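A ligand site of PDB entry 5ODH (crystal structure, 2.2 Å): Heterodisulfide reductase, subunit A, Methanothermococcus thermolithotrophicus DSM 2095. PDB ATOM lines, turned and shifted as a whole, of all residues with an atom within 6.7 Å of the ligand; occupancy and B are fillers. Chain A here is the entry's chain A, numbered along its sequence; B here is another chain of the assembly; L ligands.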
ATOM      1  N   GLN A 385      -9.080 -12.258  10.295  1.00  0.00           N
ATOM      2  CA  GLN A 385      -9.358 -12.469  11.713  1.00  0.00           C
ATOM      3  C   GLN A 385      -8.546 -13.635  12.266  1.00  0.00           C
ATOM      4  O   GLN A 385      -7.928 -14.414  11.519  1.00  0.00           O
ATOM      5  CB  GLN A 385     -10.854 -12.699  11.923  1.00  0.00           C
ATOM      6  CG  GLN A 385     -11.744 -11.542  11.446  1.00  0.00           C
ATOM      7  CD  GLN A 385     -11.321 -10.196  11.995  1.00  0.00           C
ATOM      8  OE1 GLN A 385     -10.776  -9.361  11.270  1.00  0.00           O
ATOM      9  NE2 GLN A 385     -11.567  -9.973  13.278  1.00  0.00           N
ATOM     10  N   CYS A 386      -8.533 -13.742  13.589  1.00  0.00           N
ATOM     11  CA  CYS A 386      -7.934 -14.866  14.319  1.00  0.00           C
ATOM     12  C   CYS A 386      -6.451 -15.061  13.979  1.00  0.00           C
ATOM     13  O   CYS A 386      -5.958 -16.201  13.997  1.00  0.00           O
ATOM     14  CB  CYS A 386      -8.688 -16.163  14.051  1.00  0.00           C
ATOM     15  SG  CYS A 386     -10.471 -16.074  13.991  1.00  0.00           S
ATOM     16  N   VAL A 387      -5.716 -13.998  13.701  1.00  0.00           N
ATOM     17  CA  VAL A 387      -4.290 -14.106  13.413  1.00  0.00           C
ATOM     18  C   VAL A 387      -3.545 -14.204  14.747  1.00  0.00           C
ATOM     19  O   VAL A 387      -3.515 -13.242  15.522  1.00  0.00           O
ATOM     20  CB  VAL A 387      -3.775 -12.925  12.577  1.00  0.00           C
ATOM     21  CG1 VAL A 387      -2.271 -13.052  12.358  1.00  0.00           C
ATOM     22  CG2 VAL A 387      -4.513 -12.861  11.245  1.00  0.00           C
ATOM     23  N   SER A 389      -4.466 -16.350  17.028  1.00  0.00           N
ATOM     24  CA  SER A 389      -5.451 -16.797  18.000  1.00  0.00           C
ATOM     25  C   SER A 389      -6.217 -17.971  17.402  1.00  0.00           C
ATOM     26  O   SER A 389      -6.321 -18.092  16.176  1.00  0.00           O
ATOM     27  CB  SER A 389      -6.431 -15.676  18.373  1.00  0.00           C
ATOM     28  OG  SER A 389      -5.732 -14.475  18.680  1.00  0.00           O
ATOM     29  N   ARG A 390      -6.753 -18.815  18.266  1.00  0.00           N
ATOM     30  CA  ARG A 390      -7.483 -19.999  17.822  1.00  0.00           C
ATOM     31  C   ARG A 390      -6.640 -20.803  16.828  1.00  0.00           C
ATOM     32  O   ARG A 390      -7.133 -21.280  15.808  1.00  0.00           O
ATOM     33  CB  ARG A 390      -8.822 -19.618  17.207  1.00  0.00           C
ATOM     34  CG  ARG A 390      -9.654 -18.666  18.049  1.00  0.00           C
ATOM     35  CD  ARG A 390     -10.985 -18.334  17.364  1.00  0.00           C
ATOM     36  NE  ARG A 390     -11.776 -19.521  17.080  1.00  0.00           N
ATOM     37  CZ  ARG A 390     -12.945 -19.523  16.434  1.00  0.00           C
ATOM     38  NH1 ARG A 390     -13.474 -18.385  15.995  1.00  0.00           N
ATOM     39  NH2 ARG A 390     -13.590 -20.658  16.232  1.00  0.00           N
ATOM     40  N   TYR A 398      -6.326 -19.977  22.255  1.00  0.00           N
ATOM     41  CA  TYR A 398      -7.352 -19.179  22.910  1.00  0.00           C
ATOM     42  C   TYR A 398      -7.894 -18.143  21.940  1.00  0.00           C
ATOM     43  O   TYR A 398      -7.332 -17.885  20.869  1.00  0.00           O
ATOM     44  CB  TYR A 398      -6.804 -18.493  24.159  1.00  0.00           C
ATOM     45  CG  TYR A 398      -5.571 -17.660  23.893  1.00  0.00           C
ATOM     46  CD1 TYR A 398      -4.303 -18.225  23.964  1.00  0.00           C
ATOM     47  CD2 TYR A 398      -5.667 -16.327  23.542  1.00  0.00           C
ATOM     48  CE1 TYR A 398      -3.165 -17.472  23.713  1.00  0.00           C
ATOM     49  CE2 TYR A 398      -4.542 -15.559  23.281  1.00  0.00           C
ATOM     50  CZ  TYR A 398      -3.294 -16.138  23.377  1.00  0.00           C
ATOM     51  OH  TYR A 398      -2.163 -15.392  23.125  1.00  0.00           O
ATOM     52  N   CYS A 399      -9.003 -17.553  22.354  1.00  0.00           N
ATOM     53  CA  CYS A 399      -9.628 -16.449  21.647  1.00  0.00           C
ATOM     54  C   CYS A 399      -9.155 -15.142  22.287  1.00  0.00           C
ATOM     55  O   CYS A 399      -9.101 -15.029  23.516  1.00  0.00           O
ATOM     56  CB  CYS A 399     -11.144 -16.606  21.736  1.00  0.00           C
ATOM     57  SG  CYS A 399     -12.132 -15.173  21.395  1.00  0.00           S
ATOM     58  N   SER A 400      -8.739 -14.189  21.453  1.00  0.00           N
ATOM     59  CA  SER A 400      -8.232 -12.912  21.948  1.00  0.00           C
ATOM     60  C   SER A 400      -9.329 -11.885  22.238  1.00  0.00           C
ATOM     61  O   SER A 400      -9.011 -10.756  22.634  1.00  0.00           O
ATOM     62  CB  SER A 400      -7.217 -12.320  20.953  1.00  0.00           C
ATOM     63  OG  SER A 400      -5.941 -12.885  21.121  1.00  0.00           O
ATOM     64  N   ASN A 401     -10.585 -12.223  21.995  1.00  0.00           N
ATOM     65  CA  ASN A 401     -11.732 -11.541  22.616  1.00  0.00           C
ATOM     66  C   ASN A 401     -12.124 -10.213  21.975  1.00  0.00           C
ATOM     67  O   ASN A 401     -13.318  -9.900  21.893  1.00  0.00           O
ATOM     68  CB  ASN A 401     -11.447 -11.312  24.106  1.00  0.00           C
ATOM     69  CG  ASN A 401     -12.602 -10.627  24.820  1.00  0.00           C
ATOM     70  OD1 ASN A 401     -12.726  -9.401  24.776  1.00  0.00           O
ATOM     71  ND2 ASN A 401     -13.430 -11.413  25.481  1.00  0.00           N
ATOM     72  N   VAL A 402     -11.154  -9.410  21.527  1.00  0.00           N
ATOM     73  CA  VAL A 402     -11.440  -8.063  21.039  1.00  0.00           C
ATOM     74  C   VAL A 402     -11.262  -7.908  19.542  1.00  0.00           C
ATOM     75  O   VAL A 402     -11.683  -6.880  18.990  1.00  0.00           O
ATOM     76  CB  VAL A 402     -10.581  -7.008  21.775  1.00  0.00           C
ATOM     77  CG1 VAL A 402     -10.755  -7.126  23.280  1.00  0.00           C
ATOM     78  CG2 VAL A 402      -9.117  -7.132  21.387  1.00  0.00           C
ATOM     79  N   CYS A 403     -10.644  -8.883  18.862  1.00  0.00           N
ATOM     80  CA  CYS A 403     -10.232  -8.653  17.474  1.00  0.00           C
ATOM     81  C   CYS A 403     -11.420  -8.573  16.526  1.00  0.00           C
ATOM     82  O   CYS A 403     -11.379  -7.831  15.544  1.00  0.00           O
ATOM     83  CB  CYS A 403      -9.273  -9.752  17.023  1.00  0.00           C
ATOM     84  SG  CYS A 403      -8.233 -10.445  18.356  1.00  0.00           S
ATOM     85  N   CYS A 404     -12.485  -9.342  16.785  1.00  0.00           N
ATOM     86  CA  CYS A 404     -13.677  -9.227  15.959  1.00  0.00           C
ATOM     87  C   CYS A 404     -14.235  -7.813  16.012  1.00  0.00           C
ATOM     88  O   CYS A 404     -14.582  -7.234  14.980  1.00  0.00           O
ATOM     89  CB  CYS A 404     -14.738 -10.238  16.417  1.00  0.00           C
ATOM     90  SG  CYS A 404     -14.928 -11.704  15.364  1.00  0.00           S
ATOM     91  N   MET A 405     -14.300  -7.229  17.217  1.00  0.00           N
ATOM     92  CA  MET A 405     -14.891  -5.904  17.379  1.00  0.00           C
ATOM     93  C   MET A 405     -13.976  -4.797  16.866  1.00  0.00           C
ATOM     94  O   MET A 405     -14.451  -3.853  16.223  1.00  0.00           O
ATOM     95  CB  MET A 405     -15.230  -5.660  18.852  1.00  0.00           C
ATOM     96  CG  MET A 405     -16.356  -6.538  19.381  1.00  0.00           C
ATOM     97  SD  MET A 405     -17.977  -6.158  18.660  1.00  0.00           S
ATOM     98  CE  MET A 405     -18.199  -4.453  19.199  1.00  0.00           C
ATOM     99  N   TYR A 406     -12.663  -4.894  17.117  1.00  0.00           N
ATOM    100  CA  TYR A 406     -11.791  -3.815  16.667  1.00  0.00           C
ATOM    101  C   TYR A 406     -11.621  -3.845  15.147  1.00  0.00           C
ATOM    102  O   TYR A 406     -11.333  -2.815  14.537  1.00  0.00           O
ATOM    103  CB  TYR A 406     -10.429  -3.847  17.386  1.00  0.00           C
ATOM    104  CG  TYR A 406      -9.364  -4.879  16.995  1.00  0.00           C
ATOM    105  CD1 TYR A 406      -9.074  -5.189  15.664  1.00  0.00           C
ATOM    106  CD2 TYR A 406      -8.612  -5.514  17.973  1.00  0.00           C
ATOM    107  CE1 TYR A 406      -8.115  -6.102  15.328  1.00  0.00           C
ATOM    108  CE2 TYR A 406      -7.636  -6.429  17.640  1.00  0.00           C
ATOM    109  CZ  TYR A 406      -7.393  -6.724  16.313  1.00  0.00           C
ATOM    110  OH  TYR A 406      -6.428  -7.641  15.971  1.00  0.00           O
ATOM    111  N   TYR A 427     -13.469 -14.023   8.346  1.00  0.00           N
ATOM    112  CA  TYR A 427     -13.688 -14.424   9.735  1.00  0.00           C
ATOM    113  C   TYR A 427     -14.094 -15.899   9.786  1.00  0.00           C
ATOM    114  O   TYR A 427     -14.354 -16.530   8.761  1.00  0.00           O
ATOM    115  CB  TYR A 427     -14.776 -13.566  10.390  1.00  0.00           C
ATOM    116  CG  TYR A 427     -16.171 -13.972   9.964  1.00  0.00           C
ATOM    117  CD1 TYR A 427     -16.670 -13.611   8.726  1.00  0.00           C
ATOM    118  CD2 TYR A 427     -16.963 -14.744  10.793  1.00  0.00           C
ATOM    119  CE1 TYR A 427     -17.954 -13.990   8.333  1.00  0.00           C
ATOM    120  CE2 TYR A 427     -18.233 -15.139  10.409  1.00  0.00           C
ATOM    121  CZ  TYR A 427     -18.725 -14.758   9.180  1.00  0.00           C
ATOM    122  OH  TYR A 427     -19.995 -15.157   8.819  1.00  0.00           O
ATOM    123  N   MET A 428     -14.136 -16.424  11.012  1.00  0.00           N
ATOM    124  CA  MET A 428     -14.677 -17.759  11.292  1.00  0.00           C
ATOM    125  C   MET A 428     -15.938 -17.702  12.139  1.00  0.00           C
ATOM    126  O   MET A 428     -16.960 -18.299  11.777  1.00  0.00           O
ATOM    127  CB  MET A 428     -13.629 -18.613  12.012  1.00  0.00           C
ATOM    128  CG  MET A 428     -12.428 -18.950  11.168  1.00  0.00           C
ATOM    129  SD  MET A 428     -11.397 -20.184  11.974  1.00  0.00           S
ATOM    130  CE  MET A 428     -10.920 -19.312  13.466  1.00  0.00           C
ATOM    131  N   ASP A 429     -15.872 -17.034  13.280  1.00  0.00           N
ATOM    132  CA  ASP A 429     -17.060 -16.635  14.032  1.00  0.00           C
ATOM    133  C   ASP A 429     -16.955 -15.150  14.312  1.00  0.00           C
ATOM    134  O   ASP A 429     -15.893 -14.656  14.706  1.00  0.00           O
ATOM    135  CB  ASP A 429     -17.173 -17.420  15.353  1.00  0.00           C
ATOM    136  CG  ASP A 429     -17.214 -18.926  15.145  1.00  0.00           C
ATOM    137  OD1 ASP A 429     -18.306 -19.472  14.868  1.00  0.00           O
ATOM    138  OD2 ASP A 429     -16.164 -19.578  15.292  1.00  0.00           O
ATOM    139  N   ILE A 430     -18.035 -14.413  14.094  1.00  0.00           N
ATOM    140  CA  ILE A 430     -18.109 -13.037  14.581  1.00  0.00           C
ATOM    141  C   ILE A 430     -18.533 -13.101  16.037  1.00  0.00           C
ATOM    142  O   ILE A 430     -19.643 -13.570  16.350  1.00  0.00           O
ATOM    143  CB  ILE A 430     -19.073 -12.173  13.757  1.00  0.00           C
ATOM    144  CG1 ILE A 430     -18.557 -12.021  12.328  1.00  0.00           C
ATOM    145  CG2 ILE A 430     -19.248 -10.806  14.417  1.00  0.00           C
ATOM    146  CD1 ILE A 430     -17.231 -11.307  12.199  1.00  0.00           C
ATOM    147  N   ARG A 431     -17.669 -12.642  16.916  1.00  0.00           N
ATOM    148  CA  ARG A 431     -17.890 -12.702  18.353  1.00  0.00           C
ATOM    149  C   ARG A 431     -18.136 -11.268  18.823  1.00  0.00           C
ATOM    150  O   ARG A 431     -17.215 -10.548  19.190  1.00  0.00           O
ATOM    151  CB  ARG A 431     -16.707 -13.375  19.065  1.00  0.00           C
ATOM    152  CG  ARG A 431     -16.410 -14.747  18.475  1.00  0.00           C
ATOM    153  CD  ARG A 431     -15.540 -15.642  19.344  1.00  0.00           C
ATOM    154  NE  ARG A 431     -15.682 -17.034  18.924  1.00  0.00           N
ATOM    155  CZ  ARG A 431     -14.820 -17.994  19.197  1.00  0.00           C
ATOM    156  NH1 ARG A 431     -15.038 -19.224  18.759  1.00  0.00           N
ATOM    157  NH2 ARG A 431     -13.728 -17.733  19.897  1.00  0.00           N
ATOM    158  N   PHE A 433     -20.255  -9.975  21.555  1.00  0.00           N
ATOM    159  CA  PHE A 433     -20.899 -10.729  22.619  1.00  0.00           C
ATOM    160  C   PHE A 433     -21.422  -9.874  23.771  1.00  0.00           C
ATOM    161  O   PHE A 433     -22.097 -10.419  24.653  1.00  0.00           O
ATOM    162  CB  PHE A 433     -19.915 -11.771  23.189  1.00  0.00           C
ATOM    163  CG  PHE A 433     -18.549 -11.214  23.433  1.00  0.00           C
ATOM    164  CD1 PHE A 433     -18.256 -10.552  24.624  1.00  0.00           C
ATOM    165  CD2 PHE A 433     -17.565 -11.318  22.473  1.00  0.00           C
ATOM    166  CE1 PHE A 433     -16.992 -10.032  24.838  1.00  0.00           C
ATOM    167  CE2 PHE A 433     -16.298 -10.815  22.688  1.00  0.00           C
ATOM    168  CZ  PHE A 433     -16.015 -10.155  23.870  1.00  0.00           C
ATOM    169  N   SER A 492      -5.643  -9.095  11.905  1.00  0.00           N
ATOM    170  CA  SER A 492      -6.268  -8.861  13.205  1.00  0.00           C
ATOM    171  C   SER A 492      -5.538  -9.726  14.237  1.00  0.00           C
ATOM    172  O   SER A 492      -6.013 -10.767  14.682  1.00  0.00           O
ATOM    173  CB  SER A 492      -7.758  -9.172  13.163  1.00  0.00           C
ATOM    174  OG  SER A 492      -8.435  -8.291  12.280  1.00  0.00           O
ATOM    175  N   VAL A 493      -4.356  -9.247  14.622  1.00  0.00           N
ATOM    176  CA  VAL A 493      -3.502 -10.009  15.530  1.00  0.00           C
ATOM    177  C   VAL A 493      -4.133 -10.053  16.910  1.00  0.00           C
ATOM    178  O   VAL A 493      -4.854  -9.137  17.336  1.00  0.00           O
ATOM    179  CB  VAL A 493      -2.085  -9.393  15.589  1.00  0.00           C
ATOM    180  CG1 VAL A 493      -1.417  -9.488  14.232  1.00  0.00           C
ATOM    181  CG2 VAL A 493      -2.122  -7.953  16.063  1.00  0.00           C
ATOM    182  N   GLY A 494      -3.875 -11.155  17.622  1.00  0.00           N
ATOM    183  CA  GLY A 494      -4.421 -11.369  18.950  1.00  0.00           C
ATOM    184  C   GLY A 494      -3.531 -10.780  20.022  1.00  0.00           C
ATOM    185  O   GLY A 494      -2.586 -10.032  19.750  1.00  0.00           O
ATOM    186  N   ALA B 432     -17.140 -18.220  21.918  1.00  0.00           N
ATOM    187  CA  ALA B 432     -16.347 -18.742  23.035  1.00  0.00           C
ATOM    188  C   ALA B 432     -15.160 -17.797  23.192  1.00  0.00           C
ATOM    189  O   ALA B 432     -14.075 -18.034  22.669  1.00  0.00           O
ATOM    190  CB  ALA B 432     -15.916 -20.170  22.765  1.00  0.00           C
ATOM    191  N   PHE B 433     -15.381 -16.716  23.946  1.00  0.00           N
ATOM    192  CA  PHE B 433     -14.603 -15.498  23.807  1.00  0.00           C
ATOM    193  C   PHE B 433     -13.711 -15.173  24.990  1.00  0.00           C
ATOM    194  O   PHE B 433     -12.893 -14.252  24.877  1.00  0.00           O
ATOM    195  CB  PHE B 433     -15.558 -14.318  23.584  1.00  0.00           C
ATOM    196  CG  PHE B 433     -16.700 -14.324  24.516  1.00  0.00           C
ATOM    197  CD1 PHE B 433     -16.556 -13.847  25.806  1.00  0.00           C
ATOM    198  CD2 PHE B 433     -17.910 -14.860  24.133  1.00  0.00           C
ATOM    199  CE1 PHE B 433     -17.618 -13.877  26.691  1.00  0.00           C
ATOM    200  CE2 PHE B 433     -18.983 -14.893  25.009  1.00  0.00           C
ATOM    201  CZ  PHE B 433     -18.829 -14.397  26.293  1.00  0.00           C
ATOM    202  N   GLU B 438     -12.569 -20.897  24.159  1.00  0.00           N
ATOM    203  CA  GLU B 438     -12.249 -21.528  22.881  1.00  0.00           C
ATOM    204  C   GLU B 438     -11.744 -22.945  23.085  1.00  0.00           C
ATOM    205  O   GLU B 438     -12.050 -23.849  22.298  1.00  0.00           O
ATOM    206  CB  GLU B 438     -11.218 -20.694  22.127  1.00  0.00           C
ATOM    207  CG  GLU B 438     -10.762 -21.292  20.799  1.00  0.00           C
ATOM    208  CD  GLU B 438     -11.844 -21.280  19.752  1.00  0.00           C
ATOM    209  OE1 GLU B 438     -12.906 -20.701  20.002  1.00  0.00           O
ATOM    210  OE2 GLU B 438     -11.630 -21.880  18.674  1.00  0.00           O
HETATM  211 FE1  LIG L   1     -11.961 -14.549  19.030  1.00  0.00          FE
HETATM  212 FE2  LIG L   1     -13.024 -12.616  16.711  1.00  0.00          FE
HETATM  213 FE3  LIG L   1     -10.703 -14.773  16.103  1.00  0.00          FE
HETATM  214 FE4  LIG L   1     -10.118 -12.168  17.889  1.00  0.00          FE
HETATM  215  S1  LIG L   1     -11.032 -12.724  16.101  1.00  0.00           S
HETATM  216  S2  LIG L   1     -10.146 -14.253  18.043  1.00  0.00           S
HETATM  217  S3  LIG L   1     -12.066 -12.519  18.549  1.00  0.00           S
HETATM  218  S4  LIG L   1     -12.561 -14.633  17.026  1.00  0.00           S
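Gln 385 touches the ligand (NE2 to S1, 3.98 Å). Ser 389 touches the ligand. CD of Arg 390 touches FE3 of the ligand (3.8 Å). Arg 431 touches the ligand (NH2 to FE1, 3.7 Å). Ten residues have an atom within 4 Å of the ligand: Gln 385, Cys 386, Ser 389, Arg 390, Cys 399, Ser 400, Asn 401, Cys 403, Cys 404 and Arg 431. The nearest printed residue that does not touch the ligand is Asp 429 (4.1 Å).
An iron atom (FE1) of the ligand is bound by the side-chain sulfur (SG) of Cys 399, 2.5 Å away. The backbone NH (N) of Cys 386 lies close to a sulfur (S1) of the ligand. The side-chain sulfur of Cys 386 is bound to an iron atom (FE3) of the ligand. The backbone NH (N) of Cys 404 lies close to a sulfur (S3) of the ligand, 3.7 Å away. The side-chain sulfur of Cys 404 is bound to an iron atom (FE2) of the ligand (2.5 Å). FE4 of the ligand is bound by SG of Cys 403 (2.6 Å). S2 of the ligand lies close to N of Ser 400 (3.7 Å). The backbone NH (N) of Asn 401 sits close to a sulfur (S3) of the ligand, 3.8 Å away.
The side-chain sulfur (SG) of Cys 399 lies close to the backbone NH (N) of Asn 401, 3.4 Å away. The backbone carbonyl oxygen (O) of Phe 433 of chain B sits close to the side-chain sulfur (SG) of Cys 399. The side-chain amide nitrogen of Gln 385 is in hydrogen-bond range of the backbone carbonyl oxygen of Cys 403, 3.1 Å away. O of Val 493 lies close to SG of Cys 403, at 3.8 Å. OG of Ser 389 sits at hydrogen-bond distance from OG of Ser 400. ND2 of Asn 401 sits at hydrogen-bond distance from O of Phe 433 of chain B. The backbone NH of Arg 390 sits at hydrogen-bond distance from the backbone carbonyl oxygen of Tyr 398, 2.8 Å away. The side-chain amide oxygen of Gln 385 lies within hydrogen-bond range of the side-chain hydroxyl of Ser 492 (2.8 Å).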
